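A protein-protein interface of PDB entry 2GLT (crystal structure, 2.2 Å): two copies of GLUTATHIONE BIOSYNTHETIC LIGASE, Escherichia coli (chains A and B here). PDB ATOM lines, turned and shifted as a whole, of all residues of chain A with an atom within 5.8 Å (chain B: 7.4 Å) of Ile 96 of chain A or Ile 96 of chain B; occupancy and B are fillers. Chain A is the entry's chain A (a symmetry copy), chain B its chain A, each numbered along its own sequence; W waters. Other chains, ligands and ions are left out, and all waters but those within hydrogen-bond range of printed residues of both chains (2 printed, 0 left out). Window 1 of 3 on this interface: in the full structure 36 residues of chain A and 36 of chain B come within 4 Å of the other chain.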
ATOM      1  N   PHE A  91       5.120  20.196  20.783  1.00  0.00           N
ATOM      2  CA  PHE A  91       5.557  21.363  21.527  1.00  0.00           C
ATOM      3  C   PHE A  91       5.250  20.958  22.944  1.00  0.00           C
ATOM      4  O   PHE A  91       4.101  20.916  23.398  1.00  0.00           O
ATOM      5  CB  PHE A  91       4.749  22.590  21.190  1.00  0.00           C
ATOM      6  CG  PHE A  91       5.494  23.836  21.625  1.00  0.00           C
ATOM      7  CD1 PHE A  91       6.567  24.309  20.851  1.00  0.00           C
ATOM      8  CD2 PHE A  91       5.099  24.512  22.777  1.00  0.00           C
ATOM      9  CE1 PHE A  91       7.242  25.466  21.236  1.00  0.00           C
ATOM     10  CE2 PHE A  91       5.779  25.668  23.150  1.00  0.00           C
ATOM     11  CZ  PHE A  91       6.844  26.153  22.387  1.00  0.00           C
ATOM     12  N   ASP A  92       6.318  20.537  23.585  1.00  0.00           N
ATOM     13  CA  ASP A  92       6.207  19.992  24.904  1.00  0.00           C
ATOM     14  C   ASP A  92       7.108  20.750  25.848  1.00  0.00           C
ATOM     15  O   ASP A  92       7.649  21.778  25.441  1.00  0.00           O
ATOM     16  CB  ASP A  92       6.566  18.508  24.834  1.00  0.00           C
ATOM     17  CG  ASP A  92       7.930  18.089  24.281  1.00  0.00           C
ATOM     18  OD1 ASP A  92       8.765  18.914  23.897  1.00  0.00           O
ATOM     19  OD2 ASP A  92       8.157  16.882  24.242  1.00  0.00           O
ATOM     20  N   THR A  93       7.280  20.272  27.093  1.00  0.00           N
ATOM     21  CA  THR A  93       8.139  20.961  28.036  1.00  0.00           C
ATOM     22  C   THR A  93       9.595  20.840  27.589  1.00  0.00           C
ATOM     23  O   THR A  93      10.311  21.821  27.735  1.00  0.00           O
ATOM     24  CB  THR A  93       7.912  20.393  29.487  1.00  0.00           C
ATOM     25  OG1 THR A  93       7.902  18.978  29.408  1.00  0.00           O
ATOM     26  CG2 THR A  93       6.606  20.899  30.105  1.00  0.00           C
ATOM     27  N   GLU A  94      10.026  19.753  26.937  1.00  0.00           N
ATOM     28  CA  GLU A  94      11.383  19.693  26.434  1.00  0.00           C
ATOM     29  C   GLU A  94      11.748  20.738  25.387  1.00  0.00           C
ATOM     30  O   GLU A  94      12.876  21.266  25.359  1.00  0.00           O
ATOM     31  CB  GLU A  94      11.686  18.329  25.842  1.00  0.00           C
ATOM     32  CG  GLU A  94      11.996  17.272  26.882  1.00  0.00           C
ATOM     33  CD  GLU A  94      13.027  17.666  27.943  1.00  0.00           C
ATOM     34  OE1 GLU A  94      14.181  17.917  27.599  1.00  0.00           O
ATOM     35  OE2 GLU A  94      12.655  17.709  29.116  1.00  0.00           O
ATOM     36  N   PHE A  95      10.736  21.074  24.580  1.00  0.00           N
ATOM     37  CA  PHE A  95      10.869  22.071  23.548  1.00  0.00           C
ATOM     38  C   PHE A  95      10.867  23.411  24.236  1.00  0.00           C
ATOM     39  O   PHE A  95      11.618  24.288  23.822  1.00  0.00           O
ATOM     40  CB  PHE A  95       9.683  21.991  22.602  1.00  0.00           C
ATOM     41  CG  PHE A  95       9.895  22.601  21.229  1.00  0.00           C
ATOM     42  CD1 PHE A  95      10.237  23.948  21.074  1.00  0.00           C
ATOM     43  CD2 PHE A  95       9.743  21.775  20.114  1.00  0.00           C
ATOM     44  CE1 PHE A  95      10.427  24.480  19.806  1.00  0.00           C
ATOM     45  CE2 PHE A  95       9.928  22.312  18.848  1.00  0.00           C
ATOM     46  CZ  PHE A  95      10.274  23.655  18.700  1.00  0.00           C
ATOM     47  N   ILE A  96      10.029  23.615  25.271  1.00  0.00           N
ATOM     48  CA  ILE A  96      10.058  24.871  26.005  1.00  0.00           C
ATOM     49  C   ILE A  96      11.396  25.113  26.691  1.00  0.00           C
ATOM     50  O   ILE A  96      11.844  26.264  26.640  1.00  0.00           O
ATOM     51  CB  ILE A  96       8.862  24.878  26.991  1.00  0.00           C
ATOM     52  CG1 ILE A  96       7.632  25.149  26.112  1.00  0.00           C
ATOM     53  CG2 ILE A  96       8.907  25.968  28.049  1.00  0.00           C
ATOM     54  CD1 ILE A  96       6.317  24.521  26.598  1.00  0.00           C
ATOM     55  N   TYR A  97      12.073  24.073  27.230  1.00  0.00           N
ATOM     56  CA  TYR A  97      13.394  24.225  27.844  1.00  0.00           C
ATOM     57  C   TYR A  97      14.451  24.617  26.836  1.00  0.00           C
ATOM     58  O   TYR A  97      15.271  25.471  27.133  1.00  0.00           O
ATOM     59  CB  TYR A  97      13.862  22.940  28.510  1.00  0.00           C
ATOM     60  CG  TYR A  97      12.988  22.552  29.689  1.00  0.00           C
ATOM     61  CD1 TYR A  97      12.525  23.520  30.585  1.00  0.00           C
ATOM     62  CD2 TYR A  97      12.590  21.223  29.850  1.00  0.00           C
ATOM     63  CE1 TYR A  97      11.662  23.154  31.622  1.00  0.00           C
ATOM     64  CE2 TYR A  97      11.731  20.858  30.887  1.00  0.00           C
ATOM     65  CZ  TYR A  97      11.260  21.827  31.769  1.00  0.00           C
ATOM     66  OH  TYR A  97      10.347  21.492  32.761  1.00  0.00           O
ATOM     67  N   ALA A  98      14.412  24.057  25.621  1.00  0.00           N
ATOM     68  CA  ALA A  98      15.364  24.421  24.568  1.00  0.00           C
ATOM     69  C   ALA A  98      15.257  25.845  24.083  1.00  0.00           C
ATOM     70  O   ALA A  98      16.210  26.507  23.687  1.00  0.00           O
ATOM     71  CB  ALA A  98      15.180  23.507  23.392  1.00  0.00           C
ATOM     72  N   THR A  99      14.050  26.340  24.120  1.00  0.00           N
ATOM     73  CA  THR A  99      13.712  27.719  23.800  1.00  0.00           C
ATOM     74  C   THR A  99      14.405  28.677  24.799  1.00  0.00           C
ATOM     75  O   THR A  99      14.776  29.786  24.424  1.00  0.00           O
ATOM     76  CB  THR A  99      12.183  27.625  23.842  1.00  0.00           C
ATOM     77  OG1 THR A  99      11.745  27.506  22.498  1.00  0.00           O
ATOM     78  CG2 THR A  99      11.606  28.664  24.694  1.00  0.00           C
ATOM     79  N   TYR A 100      14.609  28.300  26.090  1.00  0.00           N
ATOM     80  CA  TYR A 100      15.290  29.177  27.060  1.00  0.00           C
ATOM     81  C   TYR A 100      16.808  29.249  26.789  1.00  0.00           C
ATOM     82  O   TYR A 100      17.446  30.296  26.953  1.00  0.00           O
ATOM     83  CB  TYR A 100      15.033  28.669  28.512  1.00  0.00           C
ATOM     84  CG  TYR A 100      13.581  28.656  29.018  1.00  0.00           C
ATOM     85  CD1 TYR A 100      12.737  29.764  28.924  1.00  0.00           C
ATOM     86  CD2 TYR A 100      13.112  27.495  29.617  1.00  0.00           C
ATOM     87  CE1 TYR A 100      11.442  29.697  29.420  1.00  0.00           C
ATOM     88  CE2 TYR A 100      11.819  27.420  30.113  1.00  0.00           C
ATOM     89  CZ  TYR A 100      10.998  28.523  30.008  1.00  0.00           C
ATOM     90  OH  TYR A 100       9.745  28.450  30.557  1.00  0.00           O
ATOM     91  N   ARG A 120       6.967  30.180  22.410  1.00  0.00           N
ATOM     92  CA  ARG A 120       6.241  29.948  23.661  1.00  0.00           C
ATOM     93  C   ARG A 120       4.915  30.710  23.725  1.00  0.00           C
ATOM     94  O   ARG A 120       3.948  30.227  24.314  1.00  0.00           O
ATOM     95  CB  ARG A 120       7.097  30.382  24.876  1.00  0.00           C
ATOM     96  CG  ARG A 120       8.277  29.481  25.188  1.00  0.00           C
ATOM     97  CD  ARG A 120       8.955  29.880  26.512  1.00  0.00           C
ATOM     98  NE  ARG A 120       9.229  31.317  26.574  1.00  0.00           N
ATOM     99  CZ  ARG A 120      10.411  31.914  26.357  1.00  0.00           C
ATOM    100  NH1 ARG A 120      11.519  31.280  26.035  1.00  0.00           N
ATOM    101  NH2 ARG A 120      10.507  33.222  26.527  1.00  0.00           N
ATOM    102  N   MET B  40      -9.237  24.835  37.243  1.00  0.00           N
ATOM    103  CA  MET B  40      -8.760  24.766  35.875  1.00  0.00           C
ATOM    104  C   MET B  40      -9.799  24.435  34.813  1.00  0.00           C
ATOM    105  O   MET B  40      -9.919  25.129  33.815  1.00  0.00           O
ATOM    106  CB  MET B  40      -7.663  23.750  35.826  1.00  0.00           C
ATOM    107  CG  MET B  40      -6.399  24.249  36.452  1.00  0.00           C
ATOM    108  SD  MET B  40      -5.520  25.364  35.352  1.00  0.00           S
ATOM    109  CE  MET B  40      -4.178  24.297  34.912  1.00  0.00           C
ATOM    110  N   MET B  85      -3.747  33.571  39.801  1.00  0.00           N
ATOM    111  CA  MET B  85      -3.450  32.228  39.308  1.00  0.00           C
ATOM    112  C   MET B  85      -2.656  31.551  40.407  1.00  0.00           C
ATOM    113  O   MET B  85      -1.486  31.837  40.608  1.00  0.00           O
ATOM    114  CB  MET B  85      -2.612  32.287  38.019  1.00  0.00           C
ATOM    115  CG  MET B  85      -2.242  30.923  37.465  1.00  0.00           C
ATOM    116  SD  MET B  85      -3.710  29.896  37.320  1.00  0.00           S
ATOM    117  CE  MET B  85      -3.121  28.780  36.078  1.00  0.00           C
ATOM    118  N   PRO B  90       2.827  20.581  38.713  1.00  0.00           N
ATOM    119  CA  PRO B  90       3.796  20.969  37.690  1.00  0.00           C
ATOM    120  C   PRO B  90       3.389  22.033  36.687  1.00  0.00           C
ATOM    121  O   PRO B  90       2.219  22.382  36.505  1.00  0.00           O
ATOM    122  CB  PRO B  90       4.149  19.678  37.013  1.00  0.00           C
ATOM    123  CG  PRO B  90       3.483  18.630  37.872  1.00  0.00           C
ATOM    124  CD  PRO B  90       2.221  19.304  38.376  1.00  0.00           C
ATOM    125  N   PHE B  91       4.442  22.558  36.065  1.00  0.00           N
ATOM    126  CA  PHE B  91       4.300  23.537  35.003  1.00  0.00           C
ATOM    127  C   PHE B  91       4.434  22.678  33.773  1.00  0.00           C
ATOM    128  O   PHE B  91       5.512  22.207  33.396  1.00  0.00           O
ATOM    129  CB  PHE B  91       5.416  24.550  35.008  1.00  0.00           C
ATOM    130  CG  PHE B  91       5.009  25.772  34.206  1.00  0.00           C
ATOM    131  CD1 PHE B  91       4.130  26.710  34.770  1.00  0.00           C
ATOM    132  CD2 PHE B  91       5.522  25.961  32.926  1.00  0.00           C
ATOM    133  CE1 PHE B  91       3.769  27.845  34.045  1.00  0.00           C
ATOM    134  CE2 PHE B  91       5.157  27.099  32.212  1.00  0.00           C
ATOM    135  CZ  PHE B  91       4.288  28.044  32.763  1.00  0.00           C
ATOM    136  N   ASP B  92       3.268  22.389  33.239  1.00  0.00           N
ATOM    137  CA  ASP B  92       3.180  21.481  32.135  1.00  0.00           C
ATOM    138  C   ASP B  92       2.474  22.147  30.979  1.00  0.00           C
ATOM    139  O   ASP B  92       2.240  23.353  31.054  1.00  0.00           O
ATOM    140  CB  ASP B  92       2.446  20.228  32.611  1.00  0.00           C
ATOM    141  CG  ASP B  92       1.042  20.359  33.207  1.00  0.00           C
ATOM    142  OD1 ASP B  92       0.470  21.449  33.307  1.00  0.00           O
ATOM    143  OD2 ASP B  92       0.507  19.318  33.580  1.00  0.00           O
ATOM    144  N   THR B  93       2.134  21.396  29.917  1.00  0.00           N
ATOM    145  CA  THR B  93       1.450  21.989  28.784  1.00  0.00           C
ATOM    146  C   THR B  93       0.033  22.389  29.189  1.00  0.00           C
ATOM    147  O   THR B  93      -0.405  23.440  28.742  1.00  0.00           O
ATOM    148  CB  THR B  93       1.463  20.992  27.565  1.00  0.00           C
ATOM    149  OG1 THR B  93       1.102  19.708  28.045  1.00  0.00           O
ATOM    150  CG2 THR B  93       2.832  20.938  26.879  1.00  0.00           C
ATOM    151  N   GLU B  94      -0.644  21.687  30.107  1.00  0.00           N
ATOM    152  CA  GLU B  94      -1.948  22.133  30.553  1.00  0.00           C
ATOM    153  C   GLU B  94      -1.983  23.491  31.244  1.00  0.00           C
ATOM    154  O   GLU B  94      -2.931  24.283  31.075  1.00  0.00           O
ATOM    155  CB  GLU B  94      -2.576  21.124  31.497  1.00  0.00           C
ATOM    156  CG  GLU B  94      -3.194  19.935  30.791  1.00  0.00           C
ATOM    157  CD  GLU B  94      -4.125  20.268  29.622  1.00  0.00           C
ATOM    158  OE1 GLU B  94      -5.158  20.901  29.834  1.00  0.00           O
ATOM    159  OE2 GLU B  94      -3.801  19.875  28.500  1.00  0.00           O
ATOM    160  N   PHE B  95      -0.887  23.764  31.959  1.00  0.00           N
ATOM    161  CA  PHE B  95      -0.712  25.013  32.658  1.00  0.00           C
ATOM    162  C   PHE B  95      -0.385  26.050  31.617  1.00  0.00           C
ATOM    163  O   PHE B  95      -0.861  27.175  31.733  1.00  0.00           O
ATOM    164  CB  PHE B  95       0.447  24.897  33.633  1.00  0.00           C
ATOM    165  CG  PHE B  95       0.456  25.906  34.766  1.00  0.00           C
ATOM    166  CD1 PHE B  95       0.489  27.282  34.516  1.00  0.00           C
ATOM    167  CD2 PHE B  95       0.429  25.422  36.075  1.00  0.00           C
ATOM    168  CE1 PHE B  95       0.495  28.183  35.571  1.00  0.00           C
ATOM    169  CE2 PHE B  95       0.442  26.328  37.126  1.00  0.00           C
ATOM    170  CZ  PHE B  95       0.468  27.699  36.872  1.00  0.00           C
ATOM    171  N   ILE B  96       0.436  25.721  30.601  1.00  0.00           N
ATOM    172  CA  ILE B  96       0.711  26.678  29.537  1.00  0.00           C
ATOM    173  C   ILE B  96      -0.541  27.058  28.760  1.00  0.00           C
ATOM    174  O   ILE B  96      -0.668  28.251  28.462  1.00  0.00           O
ATOM    175  CB  ILE B  96       1.828  26.088  28.638  1.00  0.00           C
ATOM    176  CG1 ILE B  96       3.119  26.264  29.450  1.00  0.00           C
ATOM    177  CG2 ILE B  96       2.030  26.802  27.313  1.00  0.00           C
ATOM    178  CD1 ILE B  96       4.202  25.199  29.216  1.00  0.00           C
ATOM    179  N   TYR B  97      -1.490  26.124  28.513  1.00  0.00           N
ATOM    180  CA  TYR B  97      -2.747  26.437  27.831  1.00  0.00           C
ATOM    181  C   TYR B  97      -3.623  27.364  28.643  1.00  0.00           C
ATOM    182  O   TYR B  97      -4.199  28.282  28.082  1.00  0.00           O
ATOM    183  CB  TYR B  97      -3.562  25.186  27.541  1.00  0.00           C
ATOM    184  CG  TYR B  97      -2.869  24.261  26.557  1.00  0.00           C
ATOM    185  CD1 TYR B  97      -2.202  24.775  25.441  1.00  0.00           C
ATOM    186  CD2 TYR B  97      -2.841  22.886  26.797  1.00  0.00           C
ATOM    187  CE1 TYR B  97      -1.507  23.915  24.586  1.00  0.00           C
ATOM    188  CE2 TYR B  97      -2.151  22.028  25.942  1.00  0.00           C
ATOM    189  CZ  TYR B  97      -1.475  22.545  24.839  1.00  0.00           C
ATOM    190  OH  TYR B  97      -0.723  21.712  24.021  1.00  0.00           O
ATOM    191  N   ALA B  98      -3.686  27.185  29.968  1.00  0.00           N
ATOM    192  CA  ALA B  98      -4.465  28.071  30.834  1.00  0.00           C
ATOM    193  C   ALA B  98      -3.969  29.494  30.897  1.00  0.00           C
ATOM    194  O   ALA B  98      -4.697  30.468  31.050  1.00  0.00           O
ATOM    195  CB  ALA B  98      -4.483  27.516  32.229  1.00  0.00           C
ATOM    196  N   THR B  99      -2.676  29.621  30.767  1.00  0.00           N
ATOM    197  CA  THR B  99      -1.974  30.894  30.694  1.00  0.00           C
ATOM    198  C   THR B  99      -2.429  31.674  29.437  1.00  0.00           C
ATOM    199  O   THR B  99      -2.479  32.900  29.465  1.00  0.00           O
ATOM    200  CB  THR B  99      -0.527  30.392  30.740  1.00  0.00           C
ATOM    201  OG1 THR B  99      -0.083  30.552  32.078  1.00  0.00           O
ATOM    202  CG2 THR B  99       0.270  30.955  29.651  1.00  0.00           C
ATOM    203  N   TYR B 100      -2.776  31.013  28.300  1.00  0.00           N
ATOM    204  CA  TYR B 100      -3.238  31.724  27.094  1.00  0.00           C
ATOM    205  C   TYR B 100      -4.672  32.267  27.273  1.00  0.00           C
ATOM    206  O   TYR B 100      -5.017  33.353  26.793  1.00  0.00           O
ATOM    207  CB  TYR B 100      -3.181  30.773  25.859  1.00  0.00           C
ATOM    208  CG  TYR B 100      -1.805  30.235  25.435  1.00  0.00           C
ATOM    209  CD1 TYR B 100      -0.696  31.059  25.241  1.00  0.00           C
ATOM    210  CD2 TYR B 100      -1.682  28.870  25.211  1.00  0.00           C
ATOM    211  CE1 TYR B 100       0.515  30.515  24.836  1.00  0.00           C
ATOM    212  CE2 TYR B 100      -0.476  28.319  24.808  1.00  0.00           C
ATOM    213  CZ  TYR B 100       0.611  29.149  24.626  1.00  0.00           C
ATOM    214  OH  TYR B 100       1.778  28.594  24.169  1.00  0.00           O
ATOM    215  N   ILE B 101      -5.506  31.518  28.028  1.00  0.00           N
ATOM    216  CA  ILE B 101      -6.895  31.920  28.344  1.00  0.00           C
ATOM    217  C   ILE B 101      -6.892  33.151  29.262  1.00  0.00           C
ATOM    218  O   ILE B 101      -7.577  34.150  28.999  1.00  0.00           O
ATOM    219  CB  ILE B 101      -7.642  30.720  29.005  1.00  0.00           C
ATOM    220  CG1 ILE B 101      -7.739  29.644  27.945  1.00  0.00           C
ATOM    221  CG2 ILE B 101      -9.052  31.078  29.511  1.00  0.00           C
ATOM    222  CD1 ILE B 101      -8.256  28.297  28.476  1.00  0.00           C
ATOM    223  N   GLU B 103      -4.436  35.251  29.512  1.00  0.00           N
ATOM    224  CA  GLU B 103      -3.903  36.325  28.729  1.00  0.00           C
ATOM    225  C   GLU B 103      -4.954  36.998  27.845  1.00  0.00           C
ATOM    226  O   GLU B 103      -4.783  38.167  27.480  1.00  0.00           O
ATOM    227  CB  GLU B 103      -2.780  35.752  27.901  1.00  0.00           C
ATOM    228  CG  GLU B 103      -1.858  36.798  27.268  1.00  0.00           C
ATOM    229  CD  GLU B 103      -0.642  36.242  26.536  1.00  0.00           C
ATOM    230  OE1 GLU B 103      -0.482  35.026  26.421  1.00  0.00           O
ATOM    231  OE2 GLU B 103       0.162  37.045  26.062  1.00  0.00           O
ATOM    232  N   PRO B 116       0.712  36.116  32.734  1.00  0.00           N
ATOM    233  CA  PRO B 116       0.775  34.865  32.015  1.00  0.00           C
ATOM    234  C   PRO B 116       2.008  34.718  31.133  1.00  0.00           C
ATOM    235  O   PRO B 116       2.599  33.631  31.084  1.00  0.00           O
ATOM    236  CB  PRO B 116      -0.535  34.822  31.253  1.00  0.00           C
ATOM    237  CG  PRO B 116      -1.463  35.635  32.084  1.00  0.00           C
ATOM    238  CD  PRO B 116      -0.560  36.795  32.480  1.00  0.00           C
ATOM    239  N   LEU B 119       4.899  33.835  33.302  1.00  0.00           N
ATOM    240  CA  LEU B 119       4.851  32.498  33.860  1.00  0.00           C
ATOM    241  C   LEU B 119       5.471  31.529  32.875  1.00  0.00           C
ATOM    242  O   LEU B 119       6.157  30.592  33.269  1.00  0.00           O
ATOM    243  CB  LEU B 119       3.411  32.071  34.148  1.00  0.00           C
ATOM    244  CG  LEU B 119       2.597  32.778  35.245  1.00  0.00           C
ATOM    245  CD1 LEU B 119       1.146  32.294  35.192  1.00  0.00           C
ATOM    246  CD2 LEU B 119       3.121  32.440  36.600  1.00  0.00           C
ATOM    247  N   ARG B 120       5.230  31.781  31.586  1.00  0.00           N
ATOM    248  CA  ARG B 120       5.820  31.019  30.483  1.00  0.00           C
ATOM    249  C   ARG B 120       7.296  31.353  30.256  1.00  0.00           C
ATOM    250  O   ARG B 120       8.078  30.485  29.868  1.00  0.00           O
ATOM    251  CB  ARG B 120       5.061  31.298  29.163  1.00  0.00           C
ATOM    252  CG  ARG B 120       3.674  30.690  29.075  1.00  0.00           C
ATOM    253  CD  ARG B 120       3.075  30.858  27.665  1.00  0.00           C
ATOM    254  NE  ARG B 120       3.186  32.237  27.187  1.00  0.00           N
ATOM    255  CZ  ARG B 120       2.214  33.161  27.177  1.00  0.00           C
ATOM    256  NH1 ARG B 120       0.990  32.960  27.623  1.00  0.00           N
ATOM    257  NH2 ARG B 120       2.458  34.342  26.638  1.00  0.00           N
ATOM    258  N   ASP B 121       7.670  32.623  30.471  1.00  0.00           N
ATOM    259  CA  ASP B 121       9.038  33.091  30.340  1.00  0.00           C
ATOM    260  C   ASP B 121       9.989  32.671  31.463  1.00  0.00           C
ATOM    261  O   ASP B 121      11.164  32.419  31.207  1.00  0.00           O
ATOM    262  CB  ASP B 121       9.108  34.610  30.277  1.00  0.00           C
ATOM    263  CG  ASP B 121       8.528  35.281  29.033  1.00  0.00           C
ATOM    264  OD1 ASP B 121       8.321  34.632  28.008  1.00  0.00           O
ATOM    265  OD2 ASP B 121       8.280  36.483  29.096  1.00  0.00           O
ATOM    266  N   ASN B 123      10.740  29.970  34.128  1.00  0.00           N
ATOM    267  CA  ASN B 123      10.692  28.652  34.739  1.00  0.00           C
ATOM    268  C   ASN B 123      11.341  28.740  36.113  1.00  0.00           C
ATOM    269  O   ASN B 123      12.388  29.374  36.224  1.00  0.00           O
ATOM    270  CB  ASN B 123      11.447  27.703  33.844  1.00  0.00           C
ATOM    271  CG  ASN B 123      11.570  26.286  34.327  1.00  0.00           C
ATOM    272  OD1 ASN B 123      12.501  25.932  35.046  1.00  0.00           O
ATOM    273  ND2 ASN B 123      10.645  25.406  33.950  1.00  0.00           N
ATOM    274  N   LEU B 126      15.142  27.158  35.510  1.00  0.00           N
ATOM    275  CA  LEU B 126      15.944  27.771  34.448  1.00  0.00           C
ATOM    276  C   LEU B 126      16.021  29.273  34.374  1.00  0.00           C
ATOM    277  O   LEU B 126      16.901  29.841  33.711  1.00  0.00           O
ATOM    278  CB  LEU B 126      15.514  27.337  33.063  1.00  0.00           C
ATOM    279  CG  LEU B 126      16.155  26.034  32.667  1.00  0.00           C
ATOM    280  CD1 LEU B 126      15.240  24.896  33.032  1.00  0.00           C
ATOM    281  CD2 LEU B 126      16.374  25.998  31.166  1.00  0.00           C
ATOM    282  N   TYR B 194      16.459  17.066  29.489  1.00  0.00           N
ATOM    283  CA  TYR B 194      17.421  17.892  30.183  1.00  0.00           C
ATOM    284  C   TYR B 194      17.247  17.689  31.687  1.00  0.00           C
ATOM    285  O   TYR B 194      16.156  17.435  32.190  1.00  0.00           O
ATOM    286  CB  TYR B 194      17.214  19.381  29.883  1.00  0.00           C
ATOM    287  CG  TYR B 194      17.370  19.794  28.424  1.00  0.00           C
ATOM    288  CD1 TYR B 194      18.638  19.797  27.829  1.00  0.00           C
ATOM    289  CD2 TYR B 194      16.241  20.108  27.667  1.00  0.00           C
ATOM    290  CE1 TYR B 194      18.776  20.064  26.471  1.00  0.00           C
ATOM    291  CE2 TYR B 194      16.373  20.385  26.309  1.00  0.00           C
ATOM    292  CZ  TYR B 194      17.639  20.341  25.724  1.00  0.00           C
ATOM    293  OH  TYR B 194      17.786  20.553  24.380  1.00  0.00           O
HETATM  294  O   HOH W   1       8.092  23.716  33.268  1.00  0.00           O
HETATM  295  O   HOH W   2       2.017  23.024  22.989  1.00  0.00           O
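The backbone NH of Tyr 194 of chain B sits close to the side-chain carboxylate of Glu 94 of chain A (3.1 Å). The side-chain carboxylate (OD1) of Asp 121 of chain B lies within salt-bridge range of the guanidinium group (NH2) of Arg 120 of chain A, at 3.0 Å. The backbone carbonyl oxygen of Arg 120 of chain B lies within hydrogen-bond range of the side-chain hydroxyl of Tyr 100 of chain A, at 2.7 Å. OH of Tyr 100 of chain B sits at hydrogen-bond distance from O of Arg 120 of chain A (2.7 Å).
Among the printed residues, pairs that only touch across the chains: Tyr 100 of chain A with Asp 121 of chain B, Tyr 97 of chain A with Asn 123 of chain B, Ile 96 of chain A with Ile 96 of chain B, Arg 120 of chain A with Arg 120 of chain B, Phe 91 of chain A with Thr 93 of chain B, Thr 93 of chain A with Phe 91 of chain B, Tyr 100 of chain A with Asn 123 of chain B, Tyr 97 of chain A with Tyr 194 of chain B, Tyr 97 of chain A with Leu 126 of chain B and Tyr 100 of chain A with Leu 126 of chain B.
Phe 91 of chain A touches Thr 93 of chain B, and with the chains exchanged Thr 93 of chain A touches Phe 91 of chain B. Ile 96 of chain A touches its own counterpart, Ile 96 of chain B. Tyr 100 of chain A touches Arg 120 of chain B, and with the chains exchanged Arg 120 of chain A touches Tyr 100 of chain B. Arg 120 of chain B touches its own counterpart, Arg 120 of chain A. Positions printed for both chains: 91, 92, 93, 94, 95, 96, 97, 98, 99, 100 and 120. Of the 14 pairs that touch across the chains among the printed residues, 6 have their exchanged pair printed and touching as well.
Printed residues of chain B within 4 Å of Ile 96 of chain A: Ile 96 (3.4 Å). Glu 94 of chain B touches none of the printed residues of chain A. Of chain A, only Ile 96 (3.4 Å) comes within 4 Å of Ile 96 of chain B. Glu 103 of chain B touches none of the printed residues of chain A. Of the printed residues of chain A, Asn 123 of chain B touches Tyr 97 (3.4 Å) and Tyr 100 (3.8 Å). Printed residues of chain A within 4 Å of Tyr 194 of chain B: Glu 94 and Tyr 97. The nearest residue of chain A that does not touch Ile 96 of chain B is Arg 120 of chain A (4.9 Å). The nearest printed residue of chain B that does not touch Tyr 100 of chain A is Leu 119 of chain B (5.0 Å).
Of the 11 printed residues of chain A, 7 touch a printed residue of chain B. Along chain A the printed residues that touch a printed residue of chain B span positions 91 to 120. Printed residues of chain B that touch a printed residue of chain A: Phe 91, Thr 93, Ile 96, Tyr 100, Arg 120, Asp 121, Asn 123, Leu 126 and Tyr 194. Hydrophobic or aromatic side chains of chain B that line the printed part of chain A: Ile 96, Tyr 100, Leu 126 and Tyr 194.
OD1 of Asp 92 of chain A lies close to N of Glu 94 of chain A (3.4 Å). OD1 of Asn 123 of chain B sits at hydrogen-bond distance from N of Leu 126 of chain B. The side-chain carboxylate of Glu 103 of chain B lies within salt-bridge range of the guanidinium group of Arg 120 of chain B (2.8 Å).
Water W1 lies within hydrogen-bond range of O of Phe 91 of chain B, ND2 of Asn 123 of chain B and OH of Tyr 97 of chain A. Water W2 bridges O of Phe 91 of chain A (3.0 Å) and OH of Tyr 97 of chain B (3.2 Å).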
